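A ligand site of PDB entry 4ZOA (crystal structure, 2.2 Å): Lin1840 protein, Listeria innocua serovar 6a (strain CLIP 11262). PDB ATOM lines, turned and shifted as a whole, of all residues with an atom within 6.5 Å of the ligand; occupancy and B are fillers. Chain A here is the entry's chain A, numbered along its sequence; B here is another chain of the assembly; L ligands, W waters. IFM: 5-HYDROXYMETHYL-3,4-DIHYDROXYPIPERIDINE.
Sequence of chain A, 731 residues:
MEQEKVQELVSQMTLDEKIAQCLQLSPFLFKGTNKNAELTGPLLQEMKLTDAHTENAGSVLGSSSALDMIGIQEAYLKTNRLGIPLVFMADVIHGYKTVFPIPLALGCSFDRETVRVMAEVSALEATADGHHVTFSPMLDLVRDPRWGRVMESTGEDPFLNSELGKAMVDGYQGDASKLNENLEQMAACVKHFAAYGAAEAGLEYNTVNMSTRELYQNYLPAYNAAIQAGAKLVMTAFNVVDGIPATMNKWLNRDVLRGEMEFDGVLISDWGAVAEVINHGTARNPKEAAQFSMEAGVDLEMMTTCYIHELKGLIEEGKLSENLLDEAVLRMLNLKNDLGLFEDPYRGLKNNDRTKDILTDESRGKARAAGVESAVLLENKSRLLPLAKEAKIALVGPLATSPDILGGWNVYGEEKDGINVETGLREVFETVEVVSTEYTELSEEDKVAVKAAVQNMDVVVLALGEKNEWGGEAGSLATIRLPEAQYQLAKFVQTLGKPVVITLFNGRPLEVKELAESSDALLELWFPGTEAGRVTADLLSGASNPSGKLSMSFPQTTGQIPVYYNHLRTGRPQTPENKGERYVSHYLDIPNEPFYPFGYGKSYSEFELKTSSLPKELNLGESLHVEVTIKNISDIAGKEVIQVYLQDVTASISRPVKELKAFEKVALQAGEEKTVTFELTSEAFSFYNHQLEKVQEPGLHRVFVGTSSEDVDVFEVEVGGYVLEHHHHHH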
ATOM      1  N   GLN A  24      17.996  23.978  -5.951  1.00  0.00           N
ATOM      2  CA  GLN A  24      17.290  23.156  -4.942  1.00  0.00           C
ATOM      3  C   GLN A  24      17.634  21.707  -5.052  1.00  0.00           C
ATOM      4  O   GLN A  24      17.608  21.166  -6.159  1.00  0.00           O
ATOM      5  CB  GLN A  24      15.760  23.302  -5.104  1.00  0.00           C
ATOM      6  CG  GLN A  24      14.849  22.737  -4.018  1.00  0.00           C
ATOM      7  CD  GLN A  24      13.366  22.974  -4.367  1.00  0.00           C
ATOM      8  OE1 GLN A  24      12.848  22.337  -5.287  1.00  0.00           O
ATOM      9  NE2 GLN A  24      12.685  23.863  -3.631  1.00  0.00           N
ATOM     10  N   THR A  40      10.559  12.685  -6.419  1.00  0.00           N
ATOM     11  CA  THR A  40       9.403  13.084  -7.207  1.00  0.00           C
ATOM     12  C   THR A  40       9.738  13.363  -8.656  1.00  0.00           C
ATOM     13  O   THR A  40       8.927  13.966  -9.391  1.00  0.00           O
ATOM     14  CB  THR A  40       8.677  14.280  -6.575  1.00  0.00           C
ATOM     15  OG1 THR A  40       9.618  15.328  -6.265  1.00  0.00           O
ATOM     16  CG2 THR A  40       7.987  13.817  -5.329  1.00  0.00           C
ATOM     17  N   GLY A  41      10.908  12.915  -9.099  1.00  0.00           N
ATOM     18  CA  GLY A  41      11.314  13.172 -10.487  1.00  0.00           C
ATOM     19  C   GLY A  41      12.495  12.280 -10.824  1.00  0.00           C
ATOM     20  O   GLY A  41      13.087  11.722  -9.941  1.00  0.00           O
ATOM     21  N   LEU A  61      14.025  20.233  -1.042  1.00  0.00           N
ATOM     22  CA  LEU A  61      12.694  19.762  -1.334  1.00  0.00           C
ATOM     23  C   LEU A  61      12.591  18.310  -0.922  1.00  0.00           C
ATOM     24  O   LEU A  61      13.439  17.484  -1.235  1.00  0.00           O
ATOM     25  CB  LEU A  61      12.314  19.975  -2.828  1.00  0.00           C
ATOM     26  CG  LEU A  61      11.933  18.772  -3.720  1.00  0.00           C
ATOM     27  CD1 LEU A  61      11.118  19.113  -4.973  1.00  0.00           C
ATOM     28  CD2 LEU A  61      13.253  18.141  -4.104  1.00  0.00           C
ATOM     29  N   ASP A  91       5.601  18.745  -1.075  1.00  0.00           N
ATOM     30  CA  ASP A  91       4.328  18.450  -1.731  1.00  0.00           C
ATOM     31  C   ASP A  91       3.246  18.155  -0.711  1.00  0.00           C
ATOM     32  O   ASP A  91       3.093  17.021  -0.239  1.00  0.00           O
ATOM     33  CB  ASP A  91       4.526  17.257  -2.700  1.00  0.00           C
ATOM     34  CG  ASP A  91       5.323  17.648  -3.915  1.00  0.00           C
ATOM     35  OD1 ASP A  91       4.887  18.578  -4.600  1.00  0.00           O
ATOM     36  OD2 ASP A  91       6.376  17.061  -4.192  1.00  0.00           O
ATOM     37  N   ILE A  93      -0.555  18.354  -0.920  1.00  0.00           N
ATOM     38  CA  ILE A  93      -1.481  18.544  -2.008  1.00  0.00           C
ATOM     39  C   ILE A  93      -2.875  18.434  -1.497  1.00  0.00           C
ATOM     40  O   ILE A  93      -3.752  19.228  -1.821  1.00  0.00           O
ATOM     41  CB  ILE A  93      -1.257  17.482  -3.113  1.00  0.00           C
ATOM     42  CG1 ILE A  93       0.224  17.433  -3.439  1.00  0.00           C
ATOM     43  CG2 ILE A  93      -2.087  17.790  -4.363  1.00  0.00           C
ATOM     44  CD1 ILE A  93       0.880  18.794  -3.758  1.00  0.00           C
ATOM     45  N   PHE A 135       3.921  22.875  -2.435  1.00  0.00           N
ATOM     46  CA  PHE A 135       3.719  22.872  -3.868  1.00  0.00           C
ATOM     47  C   PHE A 135       2.238  22.622  -4.191  1.00  0.00           C
ATOM     48  O   PHE A 135       1.881  21.630  -4.804  1.00  0.00           O
ATOM     49  CB  PHE A 135       4.628  21.825  -4.503  1.00  0.00           C
ATOM     50  CG  PHE A 135       6.114  22.097  -4.329  1.00  0.00           C
ATOM     51  CD1 PHE A 135       6.651  23.353  -4.565  1.00  0.00           C
ATOM     52  CD2 PHE A 135       6.971  21.045  -4.017  1.00  0.00           C
ATOM     53  CE1 PHE A 135       7.995  23.597  -4.438  1.00  0.00           C
ATOM     54  CE2 PHE A 135       8.329  21.257  -3.905  1.00  0.00           C
ATOM     55  CZ  PHE A 135       8.845  22.553  -4.091  1.00  0.00           C
ATOM     56  N   SER A 136       1.399  23.565  -3.725  1.00  0.00           N
ATOM     57  CA  SER A 136      -0.081  23.572  -3.851  1.00  0.00           C
ATOM     58  C   SER A 136      -0.559  25.052  -3.765  1.00  0.00           C
ATOM     59  O   SER A 136       0.096  25.856  -3.084  1.00  0.00           O
ATOM     60  CB  SER A 136      -0.714  22.705  -2.738  1.00  0.00           C
ATOM     61  OG  SER A 136      -2.136  22.828  -2.736  1.00  0.00           O
ATOM     62  N   MET A 138      -2.667  23.332  -7.245  1.00  0.00           N
ATOM     63  CA  MET A 138      -2.548  22.975  -8.623  1.00  0.00           C
ATOM     64  C   MET A 138      -3.803  23.563  -9.273  1.00  0.00           C
ATOM     65  O   MET A 138      -4.908  23.133  -9.017  1.00  0.00           O
ATOM     66  CB  MET A 138      -2.494  21.462  -8.720  1.00  0.00           C
ATOM     67  CG  MET A 138      -2.226  20.929 -10.108  1.00  0.00           C
ATOM     68  SD  MET A 138      -3.729  20.803 -11.097  1.00  0.00           S
ATOM     69  CE  MET A 138      -3.017  19.604 -12.252  1.00  0.00           C
ATOM     70  N   ARG A 149      -3.354  13.551 -13.955  1.00  0.00           N
ATOM     71  CA  ARG A 149      -3.204  14.616 -12.977  1.00  0.00           C
ATOM     72  C   ARG A 149      -4.478  15.362 -12.777  1.00  0.00           C
ATOM     73  O   ARG A 149      -4.472  16.344 -12.010  1.00  0.00           O
ATOM     74  CB  ARG A 149      -2.102  15.592 -13.339  1.00  0.00           C
ATOM     75  CG  ARG A 149      -0.824  14.896 -13.655  1.00  0.00           C
ATOM     76  CD  ARG A 149       0.281  15.925 -13.756  1.00  0.00           C
ATOM     77  NE  ARG A 149       0.614  16.297 -12.422  1.00  0.00           N
ATOM     78  CZ  ARG A 149       1.828  16.537 -11.945  1.00  0.00           C
ATOM     79  NH1 ARG A 149       2.859  16.558 -12.717  1.00  0.00           N
ATOM     80  NH2 ARG A 149       1.971  16.761 -10.649  1.00  0.00           N
ATOM     81  N   GLU A 152      -5.626  16.262  -9.210  1.00  0.00           N
ATOM     82  CA  GLU A 152      -5.000  17.415  -8.558  1.00  0.00           C
ATOM     83  C   GLU A 152      -5.688  18.753  -8.852  1.00  0.00           C
ATOM     84  O   GLU A 152      -5.408  19.777  -8.199  1.00  0.00           O
ATOM     85  CB  GLU A 152      -3.558  17.588  -9.080  1.00  0.00           C
ATOM     86  CG  GLU A 152      -2.537  16.567  -8.633  1.00  0.00           C
ATOM     87  CD  GLU A 152      -1.254  16.639  -9.501  1.00  0.00           C
ATOM     88  OE1 GLU A 152      -0.385  17.531  -9.266  1.00  0.00           O
ATOM     89  OE2 GLU A 152      -1.084  15.733 -10.384  1.00  0.00           O
ATOM     90  N   LYS A 191       0.972  26.011  -8.941  1.00  0.00           N
ATOM     91  CA  LYS A 191       1.542  25.241 -10.040  1.00  0.00           C
ATOM     92  C   LYS A 191       0.407  24.827 -11.020  1.00  0.00           C
ATOM     93  O   LYS A 191      -0.784  24.926 -10.651  1.00  0.00           O
ATOM     94  CB  LYS A 191       2.366  24.076  -9.496  1.00  0.00           C
ATOM     95  CG  LYS A 191       1.529  22.995  -8.893  1.00  0.00           C
ATOM     96  CD  LYS A 191       2.418  21.942  -8.274  1.00  0.00           C
ATOM     97  CE  LYS A 191       1.580  20.788  -7.760  1.00  0.00           C
ATOM     98  NZ  LYS A 191       2.398  19.786  -7.088  1.00  0.00           N
ATOM     99  N   HIS A 192       0.690  24.469 -12.278  1.00  0.00           N
ATOM    100  CA  HIS A 192       1.947  24.520 -12.956  1.00  0.00           C
ATOM    101  C   HIS A 192       1.831  25.551 -14.088  1.00  0.00           C
ATOM    102  O   HIS A 192       0.993  25.392 -14.984  1.00  0.00           O
ATOM    103  CB  HIS A 192       2.270  23.140 -13.605  1.00  0.00           C
ATOM    104  CG  HIS A 192       2.258  21.990 -12.665  1.00  0.00           C
ATOM    105  ND1 HIS A 192       1.105  21.308 -12.327  1.00  0.00           N
ATOM    106  CD2 HIS A 192       3.266  21.347 -12.007  1.00  0.00           C
ATOM    107  CE1 HIS A 192       1.388  20.343 -11.492  1.00  0.00           C
ATOM    108  NE2 HIS A 192       2.691  20.338 -11.277  1.00  0.00           N
ATOM    109  N   TYR A 196      -0.843  23.164 -18.397  1.00  0.00           N
ATOM    110  CA  TYR A 196      -0.258  21.779 -18.416  1.00  0.00           C
ATOM    111  C   TYR A 196      -1.331  20.675 -18.637  1.00  0.00           C
ATOM    112  O   TYR A 196      -1.080  19.648 -19.285  1.00  0.00           O
ATOM    113  CB  TYR A 196       0.495  21.593 -17.046  1.00  0.00           C
ATOM    114  CG  TYR A 196       1.106  20.249 -16.659  1.00  0.00           C
ATOM    115  CD1 TYR A 196       1.833  19.475 -17.581  1.00  0.00           C
ATOM    116  CD2 TYR A 196       1.123  19.847 -15.357  1.00  0.00           C
ATOM    117  CE1 TYR A 196       2.422  18.277 -17.218  1.00  0.00           C
ATOM    118  CE2 TYR A 196       1.769  18.662 -14.970  1.00  0.00           C
ATOM    119  CZ  TYR A 196       2.390  17.872 -15.921  1.00  0.00           C
ATOM    120  OH  TYR A 196       2.986  16.672 -15.582  1.00  0.00           O
ATOM    121  N   MET A 235       5.327  27.867  -9.634  1.00  0.00           N
ATOM    122  CA  MET A 235       6.151  26.802 -10.259  1.00  0.00           C
ATOM    123  C   MET A 235       5.892  26.715 -11.823  1.00  0.00           C
ATOM    124  O   MET A 235       4.747  26.768 -12.284  1.00  0.00           O
ATOM    125  CB  MET A 235       5.960  25.439  -9.515  1.00  0.00           C
ATOM    126  CG  MET A 235       6.685  24.280 -10.184  1.00  0.00           C
ATOM    127  SD  MET A 235       6.289  22.625  -9.576  1.00  0.00           S
ATOM    128  CE  MET A 235       6.945  22.788  -7.881  1.00  0.00           C
ATOM    129  N   PHE A 238       5.988  21.706 -17.155  1.00  0.00           N
ATOM    130  CA  PHE A 238       6.708  20.823 -18.089  1.00  0.00           C
ATOM    131  C   PHE A 238       6.456  21.012 -19.587  1.00  0.00           C
ATOM    132  O   PHE A 238       7.359  20.677 -20.420  1.00  0.00           O
ATOM    133  CB  PHE A 238       6.407  19.356 -17.763  1.00  0.00           C
ATOM    134  CG  PHE A 238       7.082  18.880 -16.483  1.00  0.00           C
ATOM    135  CD1 PHE A 238       8.434  19.048 -16.306  1.00  0.00           C
ATOM    136  CD2 PHE A 238       6.347  18.232 -15.489  1.00  0.00           C
ATOM    137  CE1 PHE A 238       9.065  18.581 -15.176  1.00  0.00           C
ATOM    138  CE2 PHE A 238       6.943  17.799 -14.337  1.00  0.00           C
ATOM    139  CZ  PHE A 238       8.309  17.960 -14.173  1.00  0.00           C
ATOM    140  N   ASP A 270       9.745  23.416 -12.354  1.00  0.00           N
ATOM    141  CA  ASP A 270       9.374  22.053 -11.940  1.00  0.00           C
ATOM    142  C   ASP A 270      10.648  21.137 -12.095  1.00  0.00           C
ATOM    143  O   ASP A 270      11.679  21.558 -12.635  1.00  0.00           O
ATOM    144  CB  ASP A 270       8.240  21.562 -12.812  1.00  0.00           C
ATOM    145  CG  ASP A 270       7.404  20.454 -12.195  1.00  0.00           C
ATOM    146  OD1 ASP A 270       7.870  19.745 -11.293  1.00  0.00           O
ATOM    147  OD2 ASP A 270       6.238  20.296 -12.709  1.00  0.00           O
ATOM    148  N   TRP A 271      10.524  19.901 -11.663  1.00  0.00           N
ATOM    149  CA  TRP A 271      11.618  18.953 -11.540  1.00  0.00           C
ATOM    150  C   TRP A 271      12.395  18.667 -12.843  1.00  0.00           C
ATOM    151  O   TRP A 271      11.905  18.078 -13.822  1.00  0.00           O
ATOM    152  CB  TRP A 271      11.079  17.659 -10.936  1.00  0.00           C
ATOM    153  CG  TRP A 271      12.161  16.740 -10.635  1.00  0.00           C
ATOM    154  CD1 TRP A 271      13.008  16.150 -11.537  1.00  0.00           C
ATOM    155  CD2 TRP A 271      12.575  16.291  -9.343  1.00  0.00           C
ATOM    156  NE1 TRP A 271      13.924  15.371 -10.876  1.00  0.00           N
ATOM    157  CE2 TRP A 271      13.665  15.427  -9.524  1.00  0.00           C
ATOM    158  CE3 TRP A 271      12.081  16.488  -8.042  1.00  0.00           C
ATOM    159  CZ2 TRP A 271      14.303  14.792  -8.471  1.00  0.00           C
ATOM    160  CZ3 TRP A 271      12.711  15.874  -6.992  1.00  0.00           C
ATOM    161  CH2 TRP A 271      13.836  15.035  -7.211  1.00  0.00           C
ATOM    162  N   MET A 302      15.071  23.261  -9.958  1.00  0.00           N
ATOM    163  CA  MET A 302      14.775  22.089  -9.116  1.00  0.00           C
ATOM    164  C   MET A 302      15.524  20.852  -9.573  1.00  0.00           C
ATOM    165  O   MET A 302      15.182  20.223 -10.587  1.00  0.00           O
ATOM    166  CB  MET A 302      13.299  21.815  -9.088  1.00  0.00           C
ATOM    167  CG  MET A 302      12.883  20.662  -8.167  1.00  0.00           C
ATOM    168  SD  MET A 302      11.115  20.260  -8.283  1.00  0.00           S
ATOM    169  CE  MET A 302      10.413  21.655  -7.414  1.00  0.00           C
ATOM    170  N   TRP A 409      -0.873  11.562  -4.879  1.00  0.00           N
ATOM    171  CA  TRP A 409      -0.235  12.779  -4.296  1.00  0.00           C
ATOM    172  C   TRP A 409      -0.393  12.802  -2.798  1.00  0.00           C
ATOM    173  O   TRP A 409      -0.871  13.755  -2.220  1.00  0.00           O
ATOM    174  CB  TRP A 409      -0.694  14.062  -5.006  1.00  0.00           C
ATOM    175  CG  TRP A 409       0.182  14.273  -6.196  1.00  0.00           C
ATOM    176  CD1 TRP A 409      -0.202  14.264  -7.511  1.00  0.00           C
ATOM    177  CD2 TRP A 409       1.596  14.504  -6.176  1.00  0.00           C
ATOM    178  NE1 TRP A 409       0.898  14.401  -8.299  1.00  0.00           N
ATOM    179  CE2 TRP A 409       2.017  14.584  -7.532  1.00  0.00           C
ATOM    180  CE3 TRP A 409       2.569  14.621  -5.152  1.00  0.00           C
ATOM    181  CZ2 TRP A 409       3.370  14.819  -7.900  1.00  0.00           C
ATOM    182  CZ3 TRP A 409       3.943  14.834  -5.517  1.00  0.00           C
ATOM    183  CH2 TRP A 409       4.315  14.944  -6.881  1.00  0.00           C
ATOM    184  N   GLU A 473       0.883  11.884 -11.547  1.00  0.00           N
ATOM    185  CA  GLU A 473       1.873  12.182 -12.560  1.00  0.00           C
ATOM    186  C   GLU A 473       2.294  10.909 -13.285  1.00  0.00           C
ATOM    187  O   GLU A 473       2.539   9.930 -12.643  1.00  0.00           O
ATOM    188  CB  GLU A 473       3.109  12.848 -11.954  1.00  0.00           C
ATOM    189  CG  GLU A 473       4.191  13.094 -12.980  1.00  0.00           C
ATOM    190  CD  GLU A 473       5.332  14.044 -12.521  1.00  0.00           C
ATOM    191  OE1 GLU A 473       5.165  14.749 -11.463  1.00  0.00           O
ATOM    192  OE2 GLU A 473       6.362  14.084 -13.256  1.00  0.00           O
ATOM    193  N   ARG B 572      10.188  14.969 -21.723  1.00  0.00           N
ATOM    194  CA  ARG B 572      10.595  13.651 -21.180  1.00  0.00           C
ATOM    195  C   ARG B 572      10.298  12.523 -22.146  1.00  0.00           C
ATOM    196  O   ARG B 572       9.463  11.659 -21.896  1.00  0.00           O
ATOM    197  CB  ARG B 572       9.934  13.398 -19.823  1.00  0.00           C
ATOM    198  CG  ARG B 572      10.325  14.436 -18.752  1.00  0.00           C
ATOM    199  CD  ARG B 572       9.621  14.178 -17.424  1.00  0.00           C
ATOM    200  NE  ARG B 572      10.295  14.958 -16.391  1.00  0.00           N
ATOM    201  CZ  ARG B 572      10.049  14.914 -15.097  1.00  0.00           C
ATOM    202  NH1 ARG B 572       9.097  14.131 -14.593  1.00  0.00           N
ATOM    203  NH2 ARG B 572      10.799  15.657 -14.279  1.00  0.00           N
HETATM  204  O4  IFM L   1       5.093  19.501  -7.160  1.00  0.00           O
HETATM  205  C4  IFM L   1       5.588  18.497  -8.041  1.00  0.00           C
HETATM  206  C3  IFM L   1       4.997  18.706  -9.433  1.00  0.00           C
HETATM  207  O3  IFM L   1       3.592  18.755  -9.277  1.00  0.00           O
HETATM  208  C2  IFM L   1       5.483  17.693 -10.495  1.00  0.00           C
HETATM  209  N   IFM L   1       6.927  17.497 -10.466  1.00  0.00           N
HETATM  210  C1  IFM L   1       7.545  17.412  -9.159  1.00  0.00           C
HETATM  211  C5  IFM L   1       7.099  18.564  -8.238  1.00  0.00           C
HETATM  212  C6  IFM L   1       7.865  18.561  -6.889  1.00  0.00           C
HETATM  213  O6  IFM L   1       7.856  17.290  -6.294  1.00  0.00           O
HETATM  214  O   HOH W   1       8.331  15.341 -12.006  1.00  0.00           O
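Leu 61 touches the ligand (CD1 to C6, 3.8 Å).
Phe 135 touches the ligand (CB to O4, 3.6 Å).
CE of Met 235 touches O4 of the ligand, at 3.8 Å.
CE2 of Phe 238 touches N of the ligand (3.9 Å).
Trp 271 touches the ligand.
SD of Met 302 touches C6 of the ligand (3.9 Å).
Trp 409 touches the ligand.
14 residues have an atom within 4 Å of the ligand: Thr 40, Leu 61, Asp 91, Phe 135, Arg 149, Lys 191, His 192, Met 235, Phe 238, Asp 270, Trp 271, Met 302, Trp 409 and Glu 473.
The nearest printed residue that does not touch the ligand is Glu 152 (4.2 Å).
OG1 of Thr 40 is in hydrogen-bond range of O6 of the ligand, at 2.6 Å.
The side-chain carboxylate of Asp 270 lies within salt-bridge range of a nitrogen (N) of the ligand, 2.6 Å away.
OE1 of Glu 473 lies within salt-bridge range of N of the ligand (3.4 Å).
The side-chain amino group of Lys 191 lies within hydrogen-bond range of an oxygen (O3) of the ligand, 2.7 Å away.
An oxygen (O3) of the ligand is in hydrogen-bond range of the guanidinium group (NH2) of Arg 149 (2.9 Å).
An oxygen (O6) of the ligand lies within hydrogen-bond range of the side-chain carboxylate (OD2) of Asp 91 (2.6 Å).
An oxygen (O3) of the ligand lies within hydrogen-bond range of a ring nitrogen (NE2) of His 192 (2.7 Å).
Water W1 lies within hydrogen-bond range of OE2 of Glu 473 (2.6 Å), NH1 of Arg 572 of chain B (3.0 Å), N of the ligand (3.0 Å) and O of Thr 40 (3.0 Å).
NE of Arg 149 is in salt-bridge range of OE2 of Glu 152.
OD1 of Asp 91 lies within salt-bridge range of NZ of Lys 191 (3.7 Å).
NH1 of Arg 572 of chain B is in salt-bridge range of OE2 of Glu 473 (3.0 Å).
The side-chain sulfur of Met 302 sits at hydrogen-bond distance from the backbone NH of Trp 271 (3.5 Å).
NH1 of Arg 149 sits at hydrogen-bond distance from OH of Tyr 196, 2.9 Å away.
NZ of Lys 191 lies within hydrogen-bond range of O of Phe 135, 3.0 Å away.
O of Trp 271 lies within hydrogen-bond range of NH2 of Arg 572 of chain B.
NE1 of Trp 409 lies within hydrogen-bond range of OE2 of Glu 152, at 3.2 Å.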
